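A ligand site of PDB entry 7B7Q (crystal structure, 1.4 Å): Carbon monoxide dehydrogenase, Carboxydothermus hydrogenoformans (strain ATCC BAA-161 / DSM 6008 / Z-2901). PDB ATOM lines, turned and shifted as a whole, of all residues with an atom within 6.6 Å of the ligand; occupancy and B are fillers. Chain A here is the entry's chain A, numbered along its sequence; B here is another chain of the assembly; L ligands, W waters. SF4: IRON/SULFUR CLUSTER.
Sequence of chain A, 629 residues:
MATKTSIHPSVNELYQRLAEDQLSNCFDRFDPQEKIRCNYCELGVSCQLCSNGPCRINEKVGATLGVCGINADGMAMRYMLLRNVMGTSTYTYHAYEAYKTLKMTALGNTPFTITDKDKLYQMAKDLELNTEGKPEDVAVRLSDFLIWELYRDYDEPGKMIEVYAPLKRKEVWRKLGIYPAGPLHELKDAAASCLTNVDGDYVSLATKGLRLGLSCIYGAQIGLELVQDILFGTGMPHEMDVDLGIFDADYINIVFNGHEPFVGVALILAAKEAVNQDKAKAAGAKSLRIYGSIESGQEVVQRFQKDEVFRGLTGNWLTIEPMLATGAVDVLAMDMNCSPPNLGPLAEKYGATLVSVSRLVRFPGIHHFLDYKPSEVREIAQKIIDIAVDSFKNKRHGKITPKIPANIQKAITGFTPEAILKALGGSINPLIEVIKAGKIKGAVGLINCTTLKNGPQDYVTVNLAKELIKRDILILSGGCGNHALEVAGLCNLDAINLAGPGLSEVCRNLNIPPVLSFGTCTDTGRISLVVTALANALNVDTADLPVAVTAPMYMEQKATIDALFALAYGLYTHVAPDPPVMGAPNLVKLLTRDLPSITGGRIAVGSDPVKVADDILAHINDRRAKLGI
Asn 52 touches the ligand.
Gly 66 touches the ligand.
CG2 of Ile 70 touches S2 of the ligand, 3.7 Å away.
Met 75 touches the ligand.
Hydrophobic or aromatic side chains that line the ligand: Val 67, Ile 70 and Met 75.
The nearest printed residue that does not touch the ligand is Gln 48 (4.4 Å).
Water W1 lies within hydrogen-bond range of the side-chain amide nitrogen of Asn 52 (3.0 Å), the side-chain sulfur of Met 555 of chain B (3.2 Å) and a sulfur (S4) of the ligand (3.5 Å).
The backbone NH of Cys 50 lies close to a sulfur (S3) of the ligand (3.6 Å).
SG of Cys 50 is bound to FE2 of the ligand (2.3 Å).
An iron atom (FE1) of the ligand is bound by the side-chain sulfur of Cys 55 (2.3 Å).
The side-chain sulfur of Cys 47 is bound to an iron atom (FE4) of the ligand, 2.3 Å away.
N of Cys 68 sits close to S4 of the ligand, at 3.4 Å.
An iron atom (FE3) of the ligand is bound by the side-chain sulfur (SG) of Cys 68 (2.3 Å).
OG1 of Thr 196 lies close to S1 of the ligand (3.3 Å).
A sulfur (S1) of the ligand lies close to the guanidinium group (NH2) of Arg 78 (3.4 Å).
N of Gly 53 sits close to S3 of the ligand (3.7 Å).
S4 of the ligand lies close to N of Val 67, at 3.7 Å.
S3 of the ligand sits close to N of Leu 49.
The side-chain sulfur (SG) of Cys 50 sits close to the backbone NH (N) of Asn 52 (3.5 Å).
The backbone NH (N) of Val 67 lies close to the side-chain sulfur (SG) of Cys 55, at 3.7 Å.
NH2 of Arg 78 lies close to SG of Cys 47, at 3.4 Å.
N of Leu 49 lies close to SG of Cys 47 (3.7 Å).
The side-chain sulfur of Cys 68 sits close to the backbone NH of Ile 70, at 3.6 Å.
The side-chain sulfur (SG) of Cys 194 lies within hydrogen-bond range of the backbone carbonyl oxygen (O) of Arg 78 (3.4 Å).
The backbone carbonyl oxygen of Gly 53 sits close to the guanidinium group of Arg 37 of chain B.
NH2 of Arg 37 of chain B lies within hydrogen-bond range of O of Asn 52.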
ATOM      1  N   SER A  46      -6.547  20.231  23.778  1.00  0.00           N
ATOM      2  CA  SER A  46      -6.587  18.783  23.940  1.00  0.00           C
ATOM      3  C   SER A  46      -7.533  18.188  22.901  1.00  0.00           C
ATOM      4  O   SER A  46      -8.389  18.880  22.350  1.00  0.00           O
ATOM      5  CB  SER A  46      -7.081  18.396  25.325  1.00  0.00           C
ATOM      6  OG  SER A  46      -8.432  18.727  25.463  1.00  0.00           O
ATOM      7  N   CYS A  47      -7.389  16.878  22.614  1.00  0.00           N
ATOM      8  CA  CYS A  47      -8.222  16.178  21.639  1.00  0.00           C
ATOM      9  C   CYS A  47      -8.434  14.743  22.077  1.00  0.00           C
ATOM     10  O   CYS A  47      -7.485  14.065  22.496  1.00  0.00           O
ATOM     11  CB  CYS A  47      -7.547  16.200  20.282  1.00  0.00           C
ATOM     12  SG  CYS A  47      -8.581  15.558  18.925  1.00  0.00           S
ATOM     13  N   GLN A  48      -9.673  14.258  21.930  1.00  0.00           N
ATOM     14  CA  GLN A  48     -10.057  12.884  22.269  1.00  0.00           C
ATOM     15  C   GLN A  48     -10.772  12.183  21.103  1.00  0.00           C
ATOM     16  O   GLN A  48     -11.579  11.270  21.305  1.00  0.00           O
ATOM     17  CB  GLN A  48     -10.956  12.856  23.516  1.00  0.00           C
ATOM     18  CG  GLN A  48     -10.430  13.623  24.731  1.00  0.00           C
ATOM     19  CD  GLN A  48     -10.563  15.137  24.621  1.00  0.00           C
ATOM     20  OE1 GLN A  48     -11.513  15.669  24.002  1.00  0.00           O
ATOM     21  NE2 GLN A  48      -9.647  15.858  25.225  1.00  0.00           N
ATOM     22  N   LEU A  49     -10.487  12.577  19.857  1.00  0.00           N
ATOM     23  CA  LEU A  49     -11.327  12.099  18.753  1.00  0.00           C
ATOM     24  C   LEU A  49     -10.874  10.761  18.144  1.00  0.00           C
ATOM     25  O   LEU A  49     -11.658  10.182  17.378  1.00  0.00           O
ATOM     26  CB  LEU A  49     -11.473  13.159  17.656  1.00  0.00           C
ATOM     27  CG  LEU A  49     -12.108  14.478  18.089  1.00  0.00           C
ATOM     28  CD1 LEU A  49     -12.312  15.375  16.897  1.00  0.00           C
ATOM     29  CD2 LEU A  49     -13.421  14.274  18.822  1.00  0.00           C
ATOM     30  N   CYS A  50      -9.684  10.235  18.476  1.00  0.00           N
ATOM     31  CA  CYS A  50      -9.321   8.910  17.957  1.00  0.00           C
ATOM     32  C   CYS A  50      -8.421   8.159  18.922  1.00  0.00           C
ATOM     33  O   CYS A  50      -7.922   8.726  19.915  1.00  0.00           O
ATOM     34  CB  CYS A  50      -8.657   9.004  16.565  1.00  0.00           C
ATOM     35  SG  CYS A  50      -6.888   9.349  16.531  1.00  0.00           S
ATOM     36  N   SER A  51      -8.160   6.882  18.597  1.00  0.00           N
ATOM     37  CA  SER A  51      -7.437   6.007  19.518  1.00  0.00           C
ATOM     38  C   SER A  51      -5.954   6.330  19.637  1.00  0.00           C
ATOM     39  O   SER A  51      -5.327   5.857  20.579  1.00  0.00           O
ATOM     40  CB  SER A  51      -7.616   4.544  19.149  1.00  0.00           C
ATOM     41  OG  SER A  51      -6.825   4.215  18.006  1.00  0.00           O
ATOM     42  N   ASN A  52      -5.338   7.034  18.668  1.00  0.00           N
ATOM     43  CA  ASN A  52      -3.941   7.471  18.849  1.00  0.00           C
ATOM     44  C   ASN A  52      -3.820   8.519  19.943  1.00  0.00           C
ATOM     45  O   ASN A  52      -2.702   8.776  20.392  1.00  0.00           O
ATOM     46  CB  ASN A  52      -3.348   7.997  17.533  1.00  0.00           C
ATOM     47  CG  ASN A  52      -2.689   6.918  16.679  1.00  0.00           C
ATOM     48  OD1 ASN A  52      -2.082   5.987  17.202  1.00  0.00           O
ATOM     49  ND2 ASN A  52      -2.780   7.068  15.352  1.00  0.00           N
ATOM     50  N   GLY A  53      -4.920   9.168  20.333  1.00  0.00           N
ATOM     51  CA  GLY A  53      -4.958  10.082  21.438  1.00  0.00           C
ATOM     52  C   GLY A  53      -5.092   9.350  22.763  1.00  0.00           C
ATOM     53  O   GLY A  53      -4.809   8.153  22.873  1.00  0.00           O
ATOM     54  N   PRO A  54      -5.507  10.077  23.803  1.00  0.00           N
ATOM     55  CA  PRO A  54      -5.821  11.505  23.781  1.00  0.00           C
ATOM     56  C   PRO A  54      -4.561  12.358  23.581  1.00  0.00           C
ATOM     57  O   PRO A  54      -3.486  11.989  24.047  1.00  0.00           O
ATOM     58  CB  PRO A  54      -6.446  11.745  25.156  1.00  0.00           C
ATOM     59  CG  PRO A  54      -5.783  10.727  26.024  1.00  0.00           C
ATOM     60  CD  PRO A  54      -5.591   9.511  25.167  1.00  0.00           C
ATOM     61  N   CYS A  55      -4.690  13.451  22.836  1.00  0.00           N
ATOM     62  CA  CYS A  55      -3.547  14.292  22.535  1.00  0.00           C
ATOM     63  C   CYS A  55      -3.671  15.655  23.230  1.00  0.00           C
ATOM     64  O   CYS A  55      -4.778  16.098  23.572  1.00  0.00           O
ATOM     65  CB  CYS A  55      -3.416  14.540  21.021  1.00  0.00           C
ATOM     66  SG  CYS A  55      -3.003  13.015  20.080  1.00  0.00           S
ATOM     67  N   ARG A  56      -2.521  16.311  23.386  1.00  0.00           N
ATOM     68  CA  ARG A  56      -2.390  17.638  23.961  1.00  0.00           C
ATOM     69  C   ARG A  56      -1.295  18.385  23.236  1.00  0.00           C
ATOM     70  O   ARG A  56      -0.326  17.771  22.789  1.00  0.00           O
ATOM     71  CB  ARG A  56      -1.905  17.556  25.423  1.00  0.00           C
ATOM     72  CG  ARG A  56      -2.934  17.053  26.366  1.00  0.00           C
ATOM     73  CD  ARG A  56      -2.333  16.548  27.674  1.00  0.00           C
ATOM     74  NE  ARG A  56      -3.292  16.620  28.741  1.00  0.00           N
ATOM     75  CZ  ARG A  56      -3.000  16.372  30.018  1.00  0.00           C
ATOM     76  NH1 ARG A  56      -1.788  15.964  30.404  1.00  0.00           N
ATOM     77  NH2 ARG A  56      -3.944  16.548  30.924  1.00  0.00           N
ATOM     78  N   LEU A  65       2.094  19.021  17.451  1.00  0.00           N
ATOM     79  CA  LEU A  65       1.002  18.519  16.654  1.00  0.00           C
ATOM     80  C   LEU A  65       0.438  17.283  17.331  1.00  0.00           C
ATOM     81  O   LEU A  65       1.128  16.587  18.060  1.00  0.00           O
ATOM     82  CB  LEU A  65       1.478  18.191  15.212  1.00  0.00           C
ATOM     83  CG  LEU A  65       2.158  19.317  14.403  1.00  0.00           C
ATOM     84  CD1 LEU A  65       2.640  18.771  13.070  1.00  0.00           C
ATOM     85  CD2 LEU A  65       1.259  20.525  14.195  1.00  0.00           C
ATOM     86  N   GLY A  66      -0.846  16.993  17.056  1.00  0.00           N
ATOM     87  CA  GLY A  66      -1.405  15.693  17.416  1.00  0.00           C
ATOM     88  C   GLY A  66      -0.734  14.578  16.637  1.00  0.00           C
ATOM     89  O   GLY A  66      -0.013  14.823  15.666  1.00  0.00           O
ATOM     90  N   VAL A  67      -0.944  13.316  17.060  1.00  0.00           N
ATOM     91  CA  VAL A  67      -0.303  12.208  16.358  1.00  0.00           C
ATOM     92  C   VAL A  67      -0.616  12.262  14.864  1.00  0.00           C
ATOM     93  O   VAL A  67       0.261  12.012  14.020  1.00  0.00           O
ATOM     94  CB  VAL A  67      -0.692  10.834  16.970  1.00  0.00           C
ATOM     95  CG1 VAL A  67       0.015   9.691  16.220  1.00  0.00           C
ATOM     96  CG2 VAL A  67      -0.344  10.767  18.432  1.00  0.00           C
ATOM     97  N   CYS A  68      -1.853  12.589  14.511  1.00  0.00           N
ATOM     98  CA  CYS A  68      -2.289  12.631  13.120  1.00  0.00           C
ATOM     99  C   CYS A  68      -1.675  13.774  12.317  1.00  0.00           C
ATOM    100  O   CYS A  68      -1.743  13.744  11.086  1.00  0.00           O
ATOM    101  CB  CYS A  68      -3.824  12.782  13.058  1.00  0.00           C
ATOM    102  SG  CYS A  68      -4.413  14.288  13.904  1.00  0.00           S
ATOM    103  N   GLY A  69      -1.108  14.787  12.990  1.00  0.00           N
ATOM    104  CA  GLY A  69      -0.507  15.946  12.362  1.00  0.00           C
ATOM    105  C   GLY A  69      -1.290  17.254  12.494  1.00  0.00           C
ATOM    106  O   GLY A  69      -0.848  18.277  11.945  1.00  0.00           O
ATOM    107  N   ILE A  70      -2.464  17.270  13.152  1.00  0.00           N
ATOM    108  CA  ILE A  70      -3.243  18.507  13.283  1.00  0.00           C
ATOM    109  C   ILE A  70      -2.554  19.477  14.237  1.00  0.00           C
ATOM    110  O   ILE A  70      -1.961  19.070  15.250  1.00  0.00           O
ATOM    111  CB  ILE A  70      -4.702  18.213  13.687  1.00  0.00           C
ATOM    112  CG1 ILE A  70      -5.651  19.390  13.326  1.00  0.00           C
ATOM    113  CG2 ILE A  70      -4.833  17.838  15.170  1.00  0.00           C
ATOM    114  CD1 ILE A  70      -7.126  19.074  13.452  1.00  0.00           C
ATOM    115  N   MET A  75      -7.218  21.874  15.864  1.00  0.00           N
ATOM    116  CA  MET A  75      -7.738  21.117  16.987  1.00  0.00           C
ATOM    117  C   MET A  75      -8.868  21.883  17.681  1.00  0.00           C
ATOM    118  O   MET A  75      -9.962  21.356  17.912  1.00  0.00           O
ATOM    119  CB  MET A  75      -6.597  20.828  17.955  1.00  0.00           C
ATOM    120  CG  MET A  75      -6.982  19.947  19.137  1.00  0.00           C
ATOM    121  SD  MET A  75      -5.581  19.595  20.234  1.00  0.00           S
ATOM    122  CE  MET A  75      -4.583  18.526  19.209  1.00  0.00           C
ATOM    123  N   ARG A  78     -11.999  22.539  15.321  1.00  0.00           N
ATOM    124  CA  ARG A  78     -12.711  21.299  15.026  1.00  0.00           C
ATOM    125  C   ARG A  78     -13.644  20.900  16.157  1.00  0.00           C
ATOM    126  O   ARG A  78     -14.795  20.506  15.916  1.00  0.00           O
ATOM    127  CB  ARG A  78     -11.725  20.179  14.681  1.00  0.00           C
ATOM    128  CG  ARG A  78     -12.385  18.858  14.333  1.00  0.00           C
ATOM    129  CD  ARG A  78     -11.380  17.851  13.809  1.00  0.00           C
ATOM    130  NE  ARG A  78     -10.378  17.562  14.825  1.00  0.00           N
ATOM    131  CZ  ARG A  78      -9.385  16.703  14.671  1.00  0.00           C
ATOM    132  NH1 ARG A  78      -9.267  16.019  13.541  1.00  0.00           N
ATOM    133  NH2 ARG A  78      -8.493  16.515  15.645  1.00  0.00           N
ATOM    134  N   CYS A 194     -15.388  16.692  10.860  1.00  0.00           N
ATOM    135  CA  CYS A 194     -14.671  16.625  12.142  1.00  0.00           C
ATOM    136  C   CYS A 194     -14.047  15.260  12.426  1.00  0.00           C
ATOM    137  O   CYS A 194     -13.261  15.145  13.367  1.00  0.00           O
ATOM    138  CB  CYS A 194     -15.604  16.993  13.284  1.00  0.00           C
ATOM    139  SG  CYS A 194     -16.157  18.741  13.289  1.00  0.00           S
ATOM    140  N   LEU A 195     -14.395  14.225  11.665  1.00  0.00           N
ATOM    141  CA  LEU A 195     -13.769  12.933  11.849  1.00  0.00           C
ATOM    142  C   LEU A 195     -12.261  13.060  11.600  1.00  0.00           C
ATOM    143  O   LEU A 195     -11.833  13.841  10.754  1.00  0.00           O
ATOM    144  CB  LEU A 195     -14.378  11.904  10.883  1.00  0.00           C
ATOM    145  CG  LEU A 195     -14.065  10.434  11.182  1.00  0.00           C
ATOM    146  CD1 LEU A 195     -15.195   9.767  11.916  1.00  0.00           C
ATOM    147  CD2 LEU A 195     -13.700   9.666   9.915  1.00  0.00           C
ATOM    148  N   THR A 196     -11.452  12.256  12.324  1.00  0.00           N
ATOM    149  CA  THR A 196     -10.003  12.307  12.173  1.00  0.00           C
ATOM    150  C   THR A 196      -9.593  12.186  10.706  1.00  0.00           C
ATOM    151  O   THR A 196     -10.140  11.386   9.939  1.00  0.00           O
ATOM    152  CB  THR A 196      -9.374  11.199  13.011  1.00  0.00           C
ATOM    153  OG1 THR A 196      -9.837  11.304  14.377  1.00  0.00           O
ATOM    154  CG2 THR A 196      -7.845  11.261  12.928  1.00  0.00           C
ATOM    155  N   ASN A 197      -8.620  13.013  10.314  1.00  0.00           N
ATOM    156  CA  ASN A 197      -8.010  12.943   8.976  1.00  0.00           C
ATOM    157  C   ASN A 197      -8.989  13.311   7.868  1.00  0.00           C
ATOM    158  O   ASN A 197      -8.874  12.804   6.746  1.00  0.00           O
ATOM    159  CB  ASN A 197      -7.335  11.590   8.729  1.00  0.00           C
ATOM    160  CG  ASN A 197      -6.133  11.357   9.624  1.00  0.00           C
ATOM    161  OD1 ASN A 197      -5.427  12.291  10.026  1.00  0.00           O
ATOM    162  ND2 ASN A 197      -5.878  10.092   9.933  1.00  0.00           N
ATOM    163  N   GLN B  33       3.489  12.746  22.613  1.00  0.00           N
ATOM    164  CA  GLN B  33       2.177  12.572  23.237  1.00  0.00           C
ATOM    165  C   GLN B  33       2.234  11.568  24.387  1.00  0.00           C
ATOM    166  O   GLN B  33       1.553  11.744  25.421  1.00  0.00           O
ATOM    167  CB  GLN B  33       1.130  12.173  22.171  1.00  0.00           C
ATOM    168  CG  GLN B  33       0.883  13.246  21.115  1.00  0.00           C
ATOM    169  CD  GLN B  33       0.287  14.509  21.700  1.00  0.00           C
ATOM    170  OE1 GLN B  33      -0.362  14.474  22.748  1.00  0.00           O
ATOM    171  NE2 GLN B  33       0.434  15.627  20.984  1.00  0.00           N
ATOM    172  N   ARG B  37       0.339  11.890  28.456  1.00  0.00           N
ATOM    173  CA  ARG B  37      -1.009  11.360  28.308  1.00  0.00           C
ATOM    174  C   ARG B  37      -1.893  11.676  29.515  1.00  0.00           C
ATOM    175  O   ARG B  37      -1.516  11.407  30.652  1.00  0.00           O
ATOM    176  CB  ARG B  37      -0.976   9.840  28.130  1.00  0.00           C
ATOM    177  CG  ARG B  37      -0.307   9.358  26.882  1.00  0.00           C
ATOM    178  CD  ARG B  37      -1.069   9.760  25.634  1.00  0.00           C
ATOM    179  NE  ARG B  37      -0.522   9.043  24.480  1.00  0.00           N
ATOM    180  CZ  ARG B  37      -0.960   9.157  23.216  1.00  0.00           C
ATOM    181  NH1 ARG B  37      -0.394   8.443  22.251  1.00  0.00           N
ATOM    182  NH2 ARG B  37      -1.937   9.991  22.893  1.00  0.00           N
ATOM    183  N   TRP B 317      -3.780   3.650   6.073  1.00  0.00           N
ATOM    184  CA  TRP B 317      -3.589   5.081   6.268  1.00  0.00           C
ATOM    185  C   TRP B 317      -2.211   5.443   6.840  1.00  0.00           C
ATOM    186  O   TRP B 317      -1.686   6.525   6.534  1.00  0.00           O
ATOM    187  CB  TRP B 317      -4.740   5.689   7.071  1.00  0.00           C
ATOM    188  CG  TRP B 317      -4.576   5.668   8.560  1.00  0.00           C
ATOM    189  CD1 TRP B 317      -5.101   4.745   9.427  1.00  0.00           C
ATOM    190  CD2 TRP B 317      -3.902   6.642   9.375  1.00  0.00           C
ATOM    191  NE1 TRP B 317      -4.774   5.076  10.719  1.00  0.00           N
ATOM    192  CE2 TRP B 317      -4.038   6.239  10.707  1.00  0.00           C
ATOM    193  CE3 TRP B 317      -3.204   7.833   9.094  1.00  0.00           C
ATOM    194  CZ2 TRP B 317      -3.475   6.952  11.765  1.00  0.00           C
ATOM    195  CZ3 TRP B 317      -2.677   8.566  10.155  1.00  0.00           C
ATOM    196  CH2 TRP B 317      -2.775   8.105  11.465  1.00  0.00           C
ATOM    197  N   MET B 555      -9.186   2.857  15.086  1.00  0.00           N
ATOM    198  CA  MET B 555      -8.737   4.235  15.244  1.00  0.00           C
ATOM    199  C   MET B 555      -9.882   5.200  15.452  1.00  0.00           C
ATOM    200  O   MET B 555      -9.824   6.006  16.387  1.00  0.00           O
ATOM    201  CB  MET B 555      -7.876   4.726  14.097  1.00  0.00           C
ATOM    202  CG  MET B 555      -7.429   6.153  14.347  1.00  0.00           C
ATOM    203  SD  MET B 555      -6.194   6.677  13.210  1.00  0.00           S
ATOM    204  CE  MET B 555      -7.120   7.003  11.727  1.00  0.00           C
HETATM  205 FE1  SF4 L   1      -4.702  12.951  18.557  1.00  0.00          FE
HETATM  206 FE2  SF4 L   1      -6.570  11.503  17.165  1.00  0.00          FE
HETATM  207 FE3  SF4 L   1      -5.323  13.650  15.937  1.00  0.00          FE
HETATM  208 FE4  SF4 L   1      -7.134  14.056  17.987  1.00  0.00          FE
HETATM  209  S1  SF4 L   1      -7.619  13.199  15.947  1.00  0.00           S
HETATM  210  S2  SF4 L   1      -5.075  15.078  17.686  1.00  0.00           S
HETATM  211  S3  SF4 L   1      -6.776  12.199  19.334  1.00  0.00           S
HETATM  212  S4  SF4 L   1      -4.301  11.696  16.699  1.00  0.00           S
HETATM  213  O   HOH W   1      -4.529   9.229  14.257  1.00  0.00           O
